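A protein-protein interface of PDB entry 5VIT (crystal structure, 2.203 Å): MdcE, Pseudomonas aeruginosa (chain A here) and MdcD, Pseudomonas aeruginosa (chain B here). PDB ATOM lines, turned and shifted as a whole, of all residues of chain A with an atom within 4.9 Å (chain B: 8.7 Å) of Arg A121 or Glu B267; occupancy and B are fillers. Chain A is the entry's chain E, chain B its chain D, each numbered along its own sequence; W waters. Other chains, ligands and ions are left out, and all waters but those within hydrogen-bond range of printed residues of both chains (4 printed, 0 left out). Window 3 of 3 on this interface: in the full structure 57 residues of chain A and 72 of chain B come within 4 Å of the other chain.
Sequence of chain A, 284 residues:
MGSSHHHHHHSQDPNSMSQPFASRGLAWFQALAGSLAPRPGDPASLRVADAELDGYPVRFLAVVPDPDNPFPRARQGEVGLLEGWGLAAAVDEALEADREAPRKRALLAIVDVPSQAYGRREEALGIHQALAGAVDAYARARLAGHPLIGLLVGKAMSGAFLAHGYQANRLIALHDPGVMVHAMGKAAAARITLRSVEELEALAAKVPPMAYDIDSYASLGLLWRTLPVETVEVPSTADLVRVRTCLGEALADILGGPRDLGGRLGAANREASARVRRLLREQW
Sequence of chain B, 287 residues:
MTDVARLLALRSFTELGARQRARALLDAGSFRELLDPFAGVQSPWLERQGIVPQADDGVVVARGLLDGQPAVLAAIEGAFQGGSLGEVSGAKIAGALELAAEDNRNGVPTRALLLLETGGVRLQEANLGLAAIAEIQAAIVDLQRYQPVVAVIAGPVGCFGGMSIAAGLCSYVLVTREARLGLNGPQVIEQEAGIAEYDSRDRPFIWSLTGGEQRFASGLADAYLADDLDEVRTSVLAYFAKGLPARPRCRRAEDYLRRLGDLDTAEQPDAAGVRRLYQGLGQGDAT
The side-chain carboxylate (OE1) of Glu B197 sits at hydrogen-bond distance from the backbone NH (N) of Arg A120 (2.8 Å).
OE2 of Glu B197 lies within salt-bridge range of NH2 of Arg A121, 3.9 Å away.
NH2 of Arg B215 sits at hydrogen-bond distance from O of Glu A123 (2.8 Å).
The guanidinium group (NH1) of Arg B215 is in hydrogen-bond range of the backbone carbonyl oxygen (O) of Ala A124.
NH1 of Arg A121 lies within hydrogen-bond range of O of Thr B265 (2.7 Å).
The backbone carbonyl oxygen of Leu A125 sits at hydrogen-bond distance from the side-chain hydroxyl of Tyr B278 (2.8 Å).
Of the printed residues of chain B, Gly A119 touches Ile B189 (3.7 Å) and Glu B197 (3.7 Å).
Arg A121 touches five residues of chain B.
No residue of chain B comes within 4 Å of Glu A122.
Of the printed residues of chain B, Glu A123 touches Ile B189 (3.4 Å) and Arg B215 (2.8 Å).
Tyr B198 touches none of the printed residues of chain A.
Printed residues of chain A within 4 Å of Leu B209: Arg A120 (3.5 Å) and Ala A124 (3.9 Å).
Printed residues of chain A within 4 Å of Thr B265: Phe A71 (3.9 Å) and Arg A121 (2.7 Å).
Glu B267 touches just one residue of chain A: Arg A121.
Of the printed residues of chain A, Leu B277 touches Leu A125.
The nearest printed residue of chain A that does not touch Glu B267 is Pro A72 (7.4 Å).
The nearest printed residue of chain A that does not touch Leu B209 is Glu A123 (4.4 Å).
Of the 20 printed residues of chain B, 15 touch a printed residue of chain A.
Hydrophobic or aromatic side chains of chain B within 4 Å of the printed part of chain A: Ile B189, Phe B205, Leu B209, Leu B220, Leu B260, Leu B263, Pro B269, Val B274, Leu B277 and Tyr B278.
Among the printed residues, Asp or Glu carboxylates within 4 Å of a Lys or Arg side-chain nitrogen of the other chain: Arg A121 with Glu B197.
The side-chain carboxylate of Glu B197 sits at hydrogen-bond distance from the side-chain amide nitrogen of Gln B268, at 3.1 Å.
The backbone carbonyl oxygen (O) of Leu B209 lies within hydrogen-bond range of the guanidinium group (NH1) of Arg B215 (3.3 Å).
The backbone NH (N) of Leu B220 is in hydrogen-bond range of the backbone carbonyl oxygen (O) of Arg B215.
Water W1 lies within hydrogen-bond range of O of Ala A124 (2.6 Å) and O of Leu B209 (3.0 Å).
Water W3 bridges the backbone carbonyl oxygen of Pro B269 (2.7 Å) and the guanidinium group of Arg A120 (3.5 Å).
Water W2 lies within hydrogen-bond range of N of Arg A121 (2.8 Å), OE2 of Glu A122 (2.8 Å), N of Arg A120 (3.1 Å) and OE2 of Glu B197 (3.2 Å).
Water W4 bridges OE1 of Glu A123 (3.1 Å) and NH2 of Arg B215 (3.3 Å).
Thr B265 touches Phe A71 (CG2 to CE1, 3.9 Å).
CG2 of Ile B189 touches N of Gly A119, at 3.7 Å.
NE of Arg A120 touches CZ of Phe B205, at 3.8 Å.
Leu B209 touches Arg A120 (CD1 to CG, 3.5 Å).
O of Glu B267 touches NH1 of Arg A121, 3.8 Å away.
CD of Pro B269 touches CG of Arg A121, 3.4 Å away.
CG of Glu A123 touches CD1 of Ile B189 (3.4 Å).
O of Ala A124 touches CG1 of Val B274, 3.5 Å away.
Leu B263 touches Leu A125.
CD2 of Leu A125 touches CG2 of Val B274 (3.8 Å).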
ATOM      1  N   PHE A  71       4.649  23.400  19.321  1.00  0.00           N
ATOM      2  CA  PHE A  71       5.516  22.565  20.159  1.00  0.00           C
ATOM      3  C   PHE A  71       6.039  23.370  21.357  1.00  0.00           C
ATOM      4  O   PHE A  71       6.780  24.339  21.190  1.00  0.00           O
ATOM      5  CB  PHE A  71       6.662  21.985  19.322  1.00  0.00           C
ATOM      6  CG  PHE A  71       6.187  21.124  18.174  1.00  0.00           C
ATOM      7  CD1 PHE A  71       6.041  19.759  18.329  1.00  0.00           C
ATOM      8  CD2 PHE A  71       5.866  21.693  16.948  1.00  0.00           C
ATOM      9  CE1 PHE A  71       5.586  18.968  17.289  1.00  0.00           C
ATOM     10  CE2 PHE A  71       5.411  20.914  15.894  1.00  0.00           C
ATOM     11  CZ  PHE A  71       5.271  19.548  16.061  1.00  0.00           C
ATOM     12  N   PRO A  72       5.627  22.969  22.574  1.00  0.00           N
ATOM     13  CA  PRO A  72       5.906  23.618  23.866  1.00  0.00           C
ATOM     14  C   PRO A  72       7.379  23.766  24.188  1.00  0.00           C
ATOM     15  O   PRO A  72       7.750  24.629  24.985  1.00  0.00           O
ATOM     16  CB  PRO A  72       5.265  22.673  24.894  1.00  0.00           C
ATOM     17  CG  PRO A  72       4.291  21.862  24.129  1.00  0.00           C
ATOM     18  CD  PRO A  72       4.834  21.738  22.738  1.00  0.00           C
ATOM     19  N   LEU A  81      11.211  21.503  15.210  1.00  0.00           N
ATOM     20  CA  LEU A  81      10.685  20.837  14.022  1.00  0.00           C
ATOM     21  C   LEU A  81      10.186  21.809  12.955  1.00  0.00           C
ATOM     22  O   LEU A  81      10.521  21.679  11.768  1.00  0.00           O
ATOM     23  CB  LEU A  81       9.556  19.888  14.419  1.00  0.00           C
ATOM     24  CG  LEU A  81       9.946  18.765  15.376  1.00  0.00           C
ATOM     25  CD1 LEU A  81       8.734  18.329  16.175  1.00  0.00           C
ATOM     26  CD2 LEU A  81      10.533  17.584  14.593  1.00  0.00           C
ATOM     27  N   GLY A 119      13.265  18.023  23.505  1.00  0.00           N
ATOM     28  CA  GLY A 119      11.973  17.471  23.870  1.00  0.00           C
ATOM     29  C   GLY A 119      11.639  16.124  23.268  1.00  0.00           C
ATOM     30  O   GLY A 119      12.316  15.639  22.341  1.00  0.00           O
ATOM     31  N   ARG A 120      10.573  15.524  23.789  1.00  0.00           N
ATOM     32  CA  ARG A 120      10.143  14.199  23.357  1.00  0.00           C
ATOM     33  C   ARG A 120       9.510  14.241  21.978  1.00  0.00           C
ATOM     34  O   ARG A 120       9.770  13.373  21.142  1.00  0.00           O
ATOM     35  CB  ARG A 120       9.155  13.584  24.351  1.00  0.00           C
ATOM     36  CG  ARG A 120       8.794  12.140  24.001  1.00  0.00           C
ATOM     37  CD  ARG A 120       7.666  11.576  24.858  1.00  0.00           C
ATOM     38  NE  ARG A 120       7.819  11.922  26.265  1.00  0.00           N
ATOM     39  CZ  ARG A 120       7.129  11.355  27.246  1.00  0.00           C
ATOM     40  NH1 ARG A 120       6.256  10.400  26.965  1.00  0.00           N
ATOM     41  NH2 ARG A 120       7.324  11.731  28.506  1.00  0.00           N
ATOM     42  N   ARG A 121       8.657  15.235  21.755  1.00  0.00           N
ATOM     43  CA  ARG A 121       8.063  15.411  20.436  1.00  0.00           C
ATOM     44  C   ARG A 121       9.193  15.522  19.409  1.00  0.00           C
ATOM     45  O   ARG A 121       9.191  14.828  18.376  1.00  0.00           O
ATOM     46  CB  ARG A 121       7.152  16.651  20.395  1.00  0.00           C
ATOM     47  CG  ARG A 121       5.696  16.388  20.763  1.00  0.00           C
ATOM     48  CD  ARG A 121       4.893  17.676  21.029  1.00  0.00           C
ATOM     49  NE  ARG A 121       5.284  18.268  22.301  1.00  0.00           N
ATOM     50  CZ  ARG A 121       4.565  18.217  23.415  1.00  0.00           C
ATOM     51  NH1 ARG A 121       3.378  17.630  23.418  1.00  0.00           N
ATOM     52  NH2 ARG A 121       5.033  18.777  24.522  1.00  0.00           N
ATOM     53  N   GLU A 122      10.170  16.369  19.738  1.00  0.00           N
ATOM     54  CA  GLU A 122      11.292  16.682  18.853  1.00  0.00           C
ATOM     55  C   GLU A 122      12.025  15.425  18.424  1.00  0.00           C
ATOM     56  O   GLU A 122      12.185  15.163  17.226  1.00  0.00           O
ATOM     57  CB  GLU A 122      12.249  17.657  19.539  1.00  0.00           C
ATOM     58  CG  GLU A 122      11.711  19.095  19.661  1.00  0.00           C
ATOM     59  CD  GLU A 122      10.452  19.213  20.536  1.00  0.00           C
ATOM     60  OE1 GLU A 122       9.715  20.216  20.391  1.00  0.00           O
ATOM     61  OE2 GLU A 122      10.204  18.308  21.363  1.00  0.00           O
ATOM     62  N   GLU A 123      12.424  14.609  19.394  1.00  0.00           N
ATOM     63  CA  GLU A 123      13.146  13.392  19.053  1.00  0.00           C
ATOM     64  C   GLU A 123      12.255  12.358  18.385  1.00  0.00           C
ATOM     65  O   GLU A 123      12.667  11.718  17.413  1.00  0.00           O
ATOM     66  CB  GLU A 123      13.815  12.800  20.294  1.00  0.00           C
ATOM     67  CG  GLU A 123      14.849  13.739  20.905  1.00  0.00           C
ATOM     68  CD  GLU A 123      15.985  14.118  19.949  1.00  0.00           C
ATOM     69  OE1 GLU A 123      16.267  13.363  18.982  1.00  0.00           O
ATOM     70  OE2 GLU A 123      16.614  15.175  20.183  1.00  0.00           O
ATOM     71  N   ALA A 124      11.037  12.197  18.909  1.00  0.00           N
ATOM     72  CA  ALA A 124      10.092  11.226  18.361  1.00  0.00           C
ATOM     73  C   ALA A 124       9.750  11.526  16.893  1.00  0.00           C
ATOM     74  O   ALA A 124       9.630  10.602  16.077  1.00  0.00           O
ATOM     75  CB  ALA A 124       8.813  11.186  19.213  1.00  0.00           C
ATOM     76  N   LEU A 125       9.609  12.812  16.564  1.00  0.00           N
ATOM     77  CA  LEU A 125       9.224  13.232  15.216  1.00  0.00           C
ATOM     78  C   LEU A 125      10.443  13.486  14.310  1.00  0.00           C
ATOM     79  O   LEU A 125      10.310  13.795  13.110  1.00  0.00           O
ATOM     80  CB  LEU A 125       8.336  14.474  15.304  1.00  0.00           C
ATOM     81  CG  LEU A 125       6.974  14.265  16.000  1.00  0.00           C
ATOM     82  CD1 LEU A 125       6.259  15.581  16.271  1.00  0.00           C
ATOM     83  CD2 LEU A 125       6.096  13.355  15.170  1.00  0.00           C
ATOM     84  N   GLY A 126      11.635  13.344  14.883  1.00  0.00           N
ATOM     85  CA  GLY A 126      12.857  13.443  14.104  1.00  0.00           C
ATOM     86  C   GLY A 126      13.280  14.879  13.875  1.00  0.00           C
ATOM     87  O   GLY A 126      13.371  15.328  12.738  1.00  0.00           O
ATOM     88  N   ILE B 189      18.342  16.101  27.336  1.00  0.00           N
ATOM     89  CA  ILE B 189      16.925  16.462  27.261  1.00  0.00           C
ATOM     90  C   ILE B 189      16.309  16.385  28.646  1.00  0.00           C
ATOM     91  O   ILE B 189      15.547  17.266  29.045  1.00  0.00           O
ATOM     92  CB  ILE B 189      16.117  15.549  26.314  1.00  0.00           C
ATOM     93  CG1 ILE B 189      16.730  15.532  24.920  1.00  0.00           C
ATOM     94  CG2 ILE B 189      14.655  16.006  26.236  1.00  0.00           C
ATOM     95  CD1 ILE B 189      16.065  14.550  24.018  1.00  0.00           C
ATOM     96  N   GLU B 197       9.559  15.095  30.740  1.00  0.00           N
ATOM     97  CA  GLU B 197       9.740  15.141  29.289  1.00  0.00           C
ATOM     98  C   GLU B 197      10.398  13.875  28.782  1.00  0.00           C
ATOM     99  O   GLU B 197       9.967  13.294  27.782  1.00  0.00           O
ATOM    100  CB  GLU B 197      10.591  16.347  28.866  1.00  0.00           C
ATOM    101  CG  GLU B 197       9.812  17.519  28.246  1.00  0.00           C
ATOM    102  CD  GLU B 197       9.160  17.205  26.898  1.00  0.00           C
ATOM    103  OE1 GLU B 197       9.490  16.186  26.262  1.00  0.00           O
ATOM    104  OE2 GLU B 197       8.309  18.002  26.461  1.00  0.00           O
ATOM    105  N   TYR B 198      11.440  13.447  29.482  1.00  0.00           N
ATOM    106  CA  TYR B 198      12.351  12.447  28.941  1.00  0.00           C
ATOM    107  C   TYR B 198      13.111  11.785  30.085  1.00  0.00           C
ATOM    108  O   TYR B 198      13.801  12.454  30.849  1.00  0.00           O
ATOM    109  CB  TYR B 198      13.325  13.105  27.935  1.00  0.00           C
ATOM    110  CG  TYR B 198      13.660  12.286  26.693  1.00  0.00           C
ATOM    111  CD1 TYR B 198      12.759  12.179  25.638  1.00  0.00           C
ATOM    112  CD2 TYR B 198      14.895  11.653  26.557  1.00  0.00           C
ATOM    113  CE1 TYR B 198      13.069  11.441  24.489  1.00  0.00           C
ATOM    114  CE2 TYR B 198      15.208  10.916  25.412  1.00  0.00           C
ATOM    115  CZ  TYR B 198      14.291  10.815  24.380  1.00  0.00           C
ATOM    116  OH  TYR B 198      14.589  10.081  23.245  1.00  0.00           O
ATOM    117  N   PHE B 205      12.093   2.875  26.548  1.00  0.00           N
ATOM    118  CA  PHE B 205      11.443   4.102  26.100  1.00  0.00           C
ATOM    119  C   PHE B 205      12.266   4.811  25.018  1.00  0.00           C
ATOM    120  O   PHE B 205      11.763   5.104  23.925  1.00  0.00           O
ATOM    121  CB  PHE B 205      11.220   5.025  27.295  1.00  0.00           C
ATOM    122  CG  PHE B 205      10.932   6.450  26.935  1.00  0.00           C
ATOM    123  CD1 PHE B 205       9.718   6.808  26.363  1.00  0.00           C
ATOM    124  CD2 PHE B 205      11.862   7.446  27.200  1.00  0.00           C
ATOM    125  CE1 PHE B 205       9.446   8.140  26.043  1.00  0.00           C
ATOM    126  CE2 PHE B 205      11.599   8.778  26.882  1.00  0.00           C
ATOM    127  CZ  PHE B 205      10.385   9.123  26.306  1.00  0.00           C
ATOM    128  N   LEU B 209      11.427   5.496  20.706  1.00  0.00           N
ATOM    129  CA  LEU B 209      11.351   6.727  19.924  1.00  0.00           C
ATOM    130  C   LEU B 209      12.514   6.900  18.935  1.00  0.00           C
ATOM    131  O   LEU B 209      12.319   7.370  17.815  1.00  0.00           O
ATOM    132  CB  LEU B 209      11.297   7.935  20.857  1.00  0.00           C
ATOM    133  CG  LEU B 209      10.135   7.911  21.855  1.00  0.00           C
ATOM    134  CD1 LEU B 209      10.152   9.156  22.721  1.00  0.00           C
ATOM    135  CD2 LEU B 209       8.800   7.775  21.128  1.00  0.00           C
ATOM    136  N   THR B 210      13.725   6.539  19.337  1.00  0.00           N
ATOM    137  CA  THR B 210      14.896   6.931  18.553  1.00  0.00           C
ATOM    138  C   THR B 210      15.671   5.731  18.000  1.00  0.00           C
ATOM    139  O   THR B 210      16.668   5.900  17.300  1.00  0.00           O
ATOM    140  CB  THR B 210      15.833   7.814  19.396  1.00  0.00           C
ATOM    141  OG1 THR B 210      16.424   7.024  20.440  1.00  0.00           O
ATOM    142  CG2 THR B 210      15.052   8.971  20.024  1.00  0.00           C
ATOM    143  N   ARG B 215      12.748   4.292  13.599  1.00  0.00           N
ATOM    144  CA  ARG B 215      13.144   5.229  12.548  1.00  0.00           C
ATOM    145  C   ARG B 215      12.802   4.676  11.160  1.00  0.00           C
ATOM    146  O   ARG B 215      12.233   5.373  10.317  1.00  0.00           O
ATOM    147  CB  ARG B 215      14.644   5.551  12.626  1.00  0.00           C
ATOM    148  CG  ARG B 215      15.078   6.346  13.856  1.00  0.00           C
ATOM    149  CD  ARG B 215      14.210   7.582  14.094  1.00  0.00           C
ATOM    150  NE  ARG B 215      14.828   8.544  15.003  1.00  0.00           N
ATOM    151  CZ  ARG B 215      14.183   9.529  15.630  1.00  0.00           C
ATOM    152  NH1 ARG B 215      12.871   9.690  15.466  1.00  0.00           N
ATOM    153  NH2 ARG B 215      14.852  10.357  16.431  1.00  0.00           N
ATOM    154  N   LEU B 220      12.089   7.524   8.679  1.00  0.00           N
ATOM    155  CA  LEU B 220      13.254   8.368   8.907  1.00  0.00           C
ATOM    156  C   LEU B 220      14.537   7.595   8.607  1.00  0.00           C
ATOM    157  O   LEU B 220      15.637   8.141   8.691  1.00  0.00           O
ATOM    158  CB  LEU B 220      13.253   8.916  10.338  1.00  0.00           C
ATOM    159  CG  LEU B 220      12.054   9.841  10.577  1.00  0.00           C
ATOM    160  CD1 LEU B 220      12.024  10.462  11.985  1.00  0.00           C
ATOM    161  CD2 LEU B 220      12.013  10.919   9.503  1.00  0.00           C
ATOM    162  N   LEU B 260       2.839  17.741  10.245  1.00  0.00           N
ATOM    163  CA  LEU B 260       3.111  18.299  11.564  1.00  0.00           C
ATOM    164  C   LEU B 260       2.008  19.277  11.966  1.00  0.00           C
ATOM    165  O   LEU B 260       1.786  19.532  13.156  1.00  0.00           O
ATOM    166  CB  LEU B 260       4.488  18.989  11.587  1.00  0.00           C
ATOM    167  CG  LEU B 260       5.717  18.063  11.543  1.00  0.00           C
ATOM    168  CD1 LEU B 260       7.018  18.857  11.398  1.00  0.00           C
ATOM    169  CD2 LEU B 260       5.780  17.177  12.775  1.00  0.00           C
ATOM    170  N   LEU B 263      -1.084  17.509  13.484  1.00  0.00           N
ATOM    171  CA  LEU B 263      -0.828  16.861  14.760  1.00  0.00           C
ATOM    172  C   LEU B 263      -1.428  17.659  15.910  1.00  0.00           C
ATOM    173  O   LEU B 263      -1.229  18.871  16.027  1.00  0.00           O
ATOM    174  CB  LEU B 263       0.679  16.666  14.981  1.00  0.00           C
ATOM    175  CG  LEU B 263       1.079  15.958  16.280  1.00  0.00           C
ATOM    176  CD1 LEU B 263       0.679  14.483  16.210  1.00  0.00           C
ATOM    177  CD2 LEU B 263       2.567  16.112  16.585  1.00  0.00           C
ATOM    178  N   ASP B 264      -2.176  16.970  16.757  1.00  0.00           N
ATOM    179  CA  ASP B 264      -2.546  17.541  18.036  1.00  0.00           C
ATOM    180  C   ASP B 264      -1.317  17.423  18.924  1.00  0.00           C
ATOM    181  O   ASP B 264      -0.942  16.324  19.336  1.00  0.00           O
ATOM    182  CB  ASP B 264      -3.747  16.818  18.653  1.00  0.00           C
ATOM    183  CG  ASP B 264      -4.450  17.650  19.713  1.00  0.00           C
ATOM    184  OD1 ASP B 264      -3.801  18.541  20.309  1.00  0.00           O
ATOM    185  OD2 ASP B 264      -5.650  17.398  19.963  1.00  0.00           O
ATOM    186  N   THR B 265      -0.674  18.548  19.204  1.00  0.00           N
ATOM    187  CA  THR B 265       0.574  18.522  19.962  1.00  0.00           C
ATOM    188  C   THR B 265       0.335  18.701  21.453  1.00  0.00           C
ATOM    189  O   THR B 265       1.285  18.860  22.227  1.00  0.00           O
ATOM    190  CB  THR B 265       1.537  19.618  19.493  1.00  0.00           C
ATOM    191  OG1 THR B 265       0.975  20.901  19.796  1.00  0.00           O
ATOM    192  CG2 THR B 265       1.805  19.503  17.987  1.00  0.00           C
ATOM    193  N   ALA B 266      -0.934  18.687  21.851  1.00  0.00           N
ATOM    194  CA  ALA B 266      -1.306  18.902  23.246  1.00  0.00           C
ATOM    195  C   ALA B 266      -0.759  17.789  24.147  1.00  0.00           C
ATOM    196  O   ALA B 266      -0.280  18.046  25.254  1.00  0.00           O
ATOM    197  CB  ALA B 266      -2.835  19.010  23.377  1.00  0.00           C
ATOM    198  N   GLU B 267      -0.823  16.553  23.667  1.00  0.00           N
ATOM    199  CA  GLU B 267      -0.305  15.420  24.424  1.00  0.00           C
ATOM    200  C   GLU B 267       0.901  14.777  23.717  1.00  0.00           C
ATOM    201  O   GLU B 267       1.041  14.845  22.487  1.00  0.00           O
ATOM    202  CB  GLU B 267      -1.416  14.382  24.668  1.00  0.00           C
ATOM    203  CG  GLU B 267      -2.484  14.811  25.701  1.00  0.00           C
ATOM    204  CD  GLU B 267      -3.848  15.142  25.083  1.00  0.00           C
ATOM    205  OE1 GLU B 267      -4.025  14.968  23.854  1.00  0.00           O
ATOM    206  OE2 GLU B 267      -4.748  15.592  25.830  1.00  0.00           O
ATOM    207  N   GLN B 268       1.772  14.158  24.510  1.00  0.00           N
ATOM    208  CA  GLN B 268       2.992  13.533  23.999  1.00  0.00           C
ATOM    209  C   GLN B 268       2.722  12.346  23.071  1.00  0.00           C
ATOM    210  O   GLN B 268       2.077  11.381  23.469  1.00  0.00           O
ATOM    211  CB  GLN B 268       3.872  13.075  25.169  1.00  0.00           C
ATOM    212  CG  GLN B 268       4.401  14.220  26.024  1.00  0.00           C
ATOM    213  CD  GLN B 268       5.675  14.841  25.458  1.00  0.00           C
ATOM    214  OE1 GLN B 268       5.934  14.783  24.249  1.00  0.00           O
ATOM    215  NE2 GLN B 268       6.472  15.441  26.334  1.00  0.00           N
ATOM    216  N   PRO B 269       3.229  12.408  21.831  1.00  0.00           N
ATOM    217  CA  PRO B 269       3.087  11.275  20.909  1.00  0.00           C
ATOM    218  C   PRO B 269       3.875  10.073  21.407  1.00  0.00           C
ATOM    219  O   PRO B 269       4.714  10.218  22.299  1.00  0.00           O
ATOM    220  CB  PRO B 269       3.671  11.807  19.604  1.00  0.00           C
ATOM    221  CG  PRO B 269       4.685  12.808  20.051  1.00  0.00           C
ATOM    222  CD  PRO B 269       4.098  13.460  21.281  1.00  0.00           C
ATOM    223  N   ASP B 270       3.596   8.905  20.843  1.00  0.00           N
ATOM    224  CA  ASP B 270       4.344   7.694  21.153  1.00  0.00           C
ATOM    225  C   ASP B 270       4.810   7.092  19.843  1.00  0.00           C
ATOM    226  O   ASP B 270       4.535   7.649  18.780  1.00  0.00           O
ATOM    227  CB  ASP B 270       3.491   6.693  21.946  1.00  0.00           C
ATOM    228  CG  ASP B 270       2.104   6.488  21.342  1.00  0.00           C
ATOM    229  OD1 ASP B 270       1.984   6.435  20.096  1.00  0.00           O
ATOM    230  OD2 ASP B 270       1.136   6.371  22.127  1.00  0.00           O
ATOM    231  N   VAL B 274       3.604   8.329  15.912  1.00  0.00           N
ATOM    232  CA  VAL B 274       4.557   8.826  14.937  1.00  0.00           C
ATOM    233  C   VAL B 274       4.473   8.007  13.653  1.00  0.00           C
ATOM    234  O   VAL B 274       4.422   8.578  12.562  1.00  0.00           O
ATOM    235  CB  VAL B 274       5.999   8.813  15.511  1.00  0.00           C
ATOM    236  CG1 VAL B 274       7.033   9.052  14.410  1.00  0.00           C
ATOM    237  CG2 VAL B 274       6.125   9.849  16.629  1.00  0.00           C
ATOM    238  N   LEU B 277       1.231   9.214  12.033  1.00  0.00           N
ATOM    239  CA  LEU B 277       1.382  10.575  11.499  1.00  0.00           C
ATOM    240  C   LEU B 277       2.138  10.623  10.165  1.00  0.00           C
ATOM    241  O   LEU B 277       1.804  11.420   9.286  1.00  0.00           O
ATOM    242  CB  LEU B 277       2.093  11.473  12.517  1.00  0.00           C
ATOM    243  CG  LEU B 277       2.190  12.933  12.072  1.00  0.00           C
ATOM    244  CD1 LEU B 277       0.805  13.441  11.695  1.00  0.00           C
ATOM    245  CD2 LEU B 277       2.817  13.822  13.143  1.00  0.00           C
ATOM    246  N   TYR B 278       3.146   9.765  10.022  1.00  0.00           N
ATOM    247  CA  TYR B 278       3.919   9.673   8.786  1.00  0.00           C
ATOM    248  C   TYR B 278       3.449   8.491   7.939  1.00  0.00           C
ATOM    249  O   TYR B 278       4.064   8.168   6.917  1.00  0.00           O
ATOM    250  CB  TYR B 278       5.423   9.533   9.079  1.00  0.00           C
ATOM    251  CG  TYR B 278       6.065  10.712   9.789  1.00  0.00           C
ATOM    252  CD1 TYR B 278       7.392  10.656  10.203  1.00  0.00           C
ATOM    253  CD2 TYR B 278       5.352  11.877  10.047  1.00  0.00           C
ATOM    254  CE1 TYR B 278       7.987  11.727  10.855  1.00  0.00           C
ATOM    255  CE2 TYR B 278       5.940  12.951  10.700  1.00  0.00           C
ATOM    256  CZ  TYR B 278       7.259  12.870  11.097  1.00  0.00           C
ATOM    257  OH  TYR B 278       7.846  13.936  11.741  1.00  0.00           O
HETATM  258  O   HOH W   1       9.659   8.085  16.754  1.00  0.00           O
HETATM  259  O   HOH W   2       8.307  17.513  23.320  1.00  0.00           O
HETATM  260  O   HOH W   3       5.766   8.543  24.097  1.00  0.00           O
HETATM  261  O   HOH W   4      15.495  13.576  16.020  1.00  0.00           O
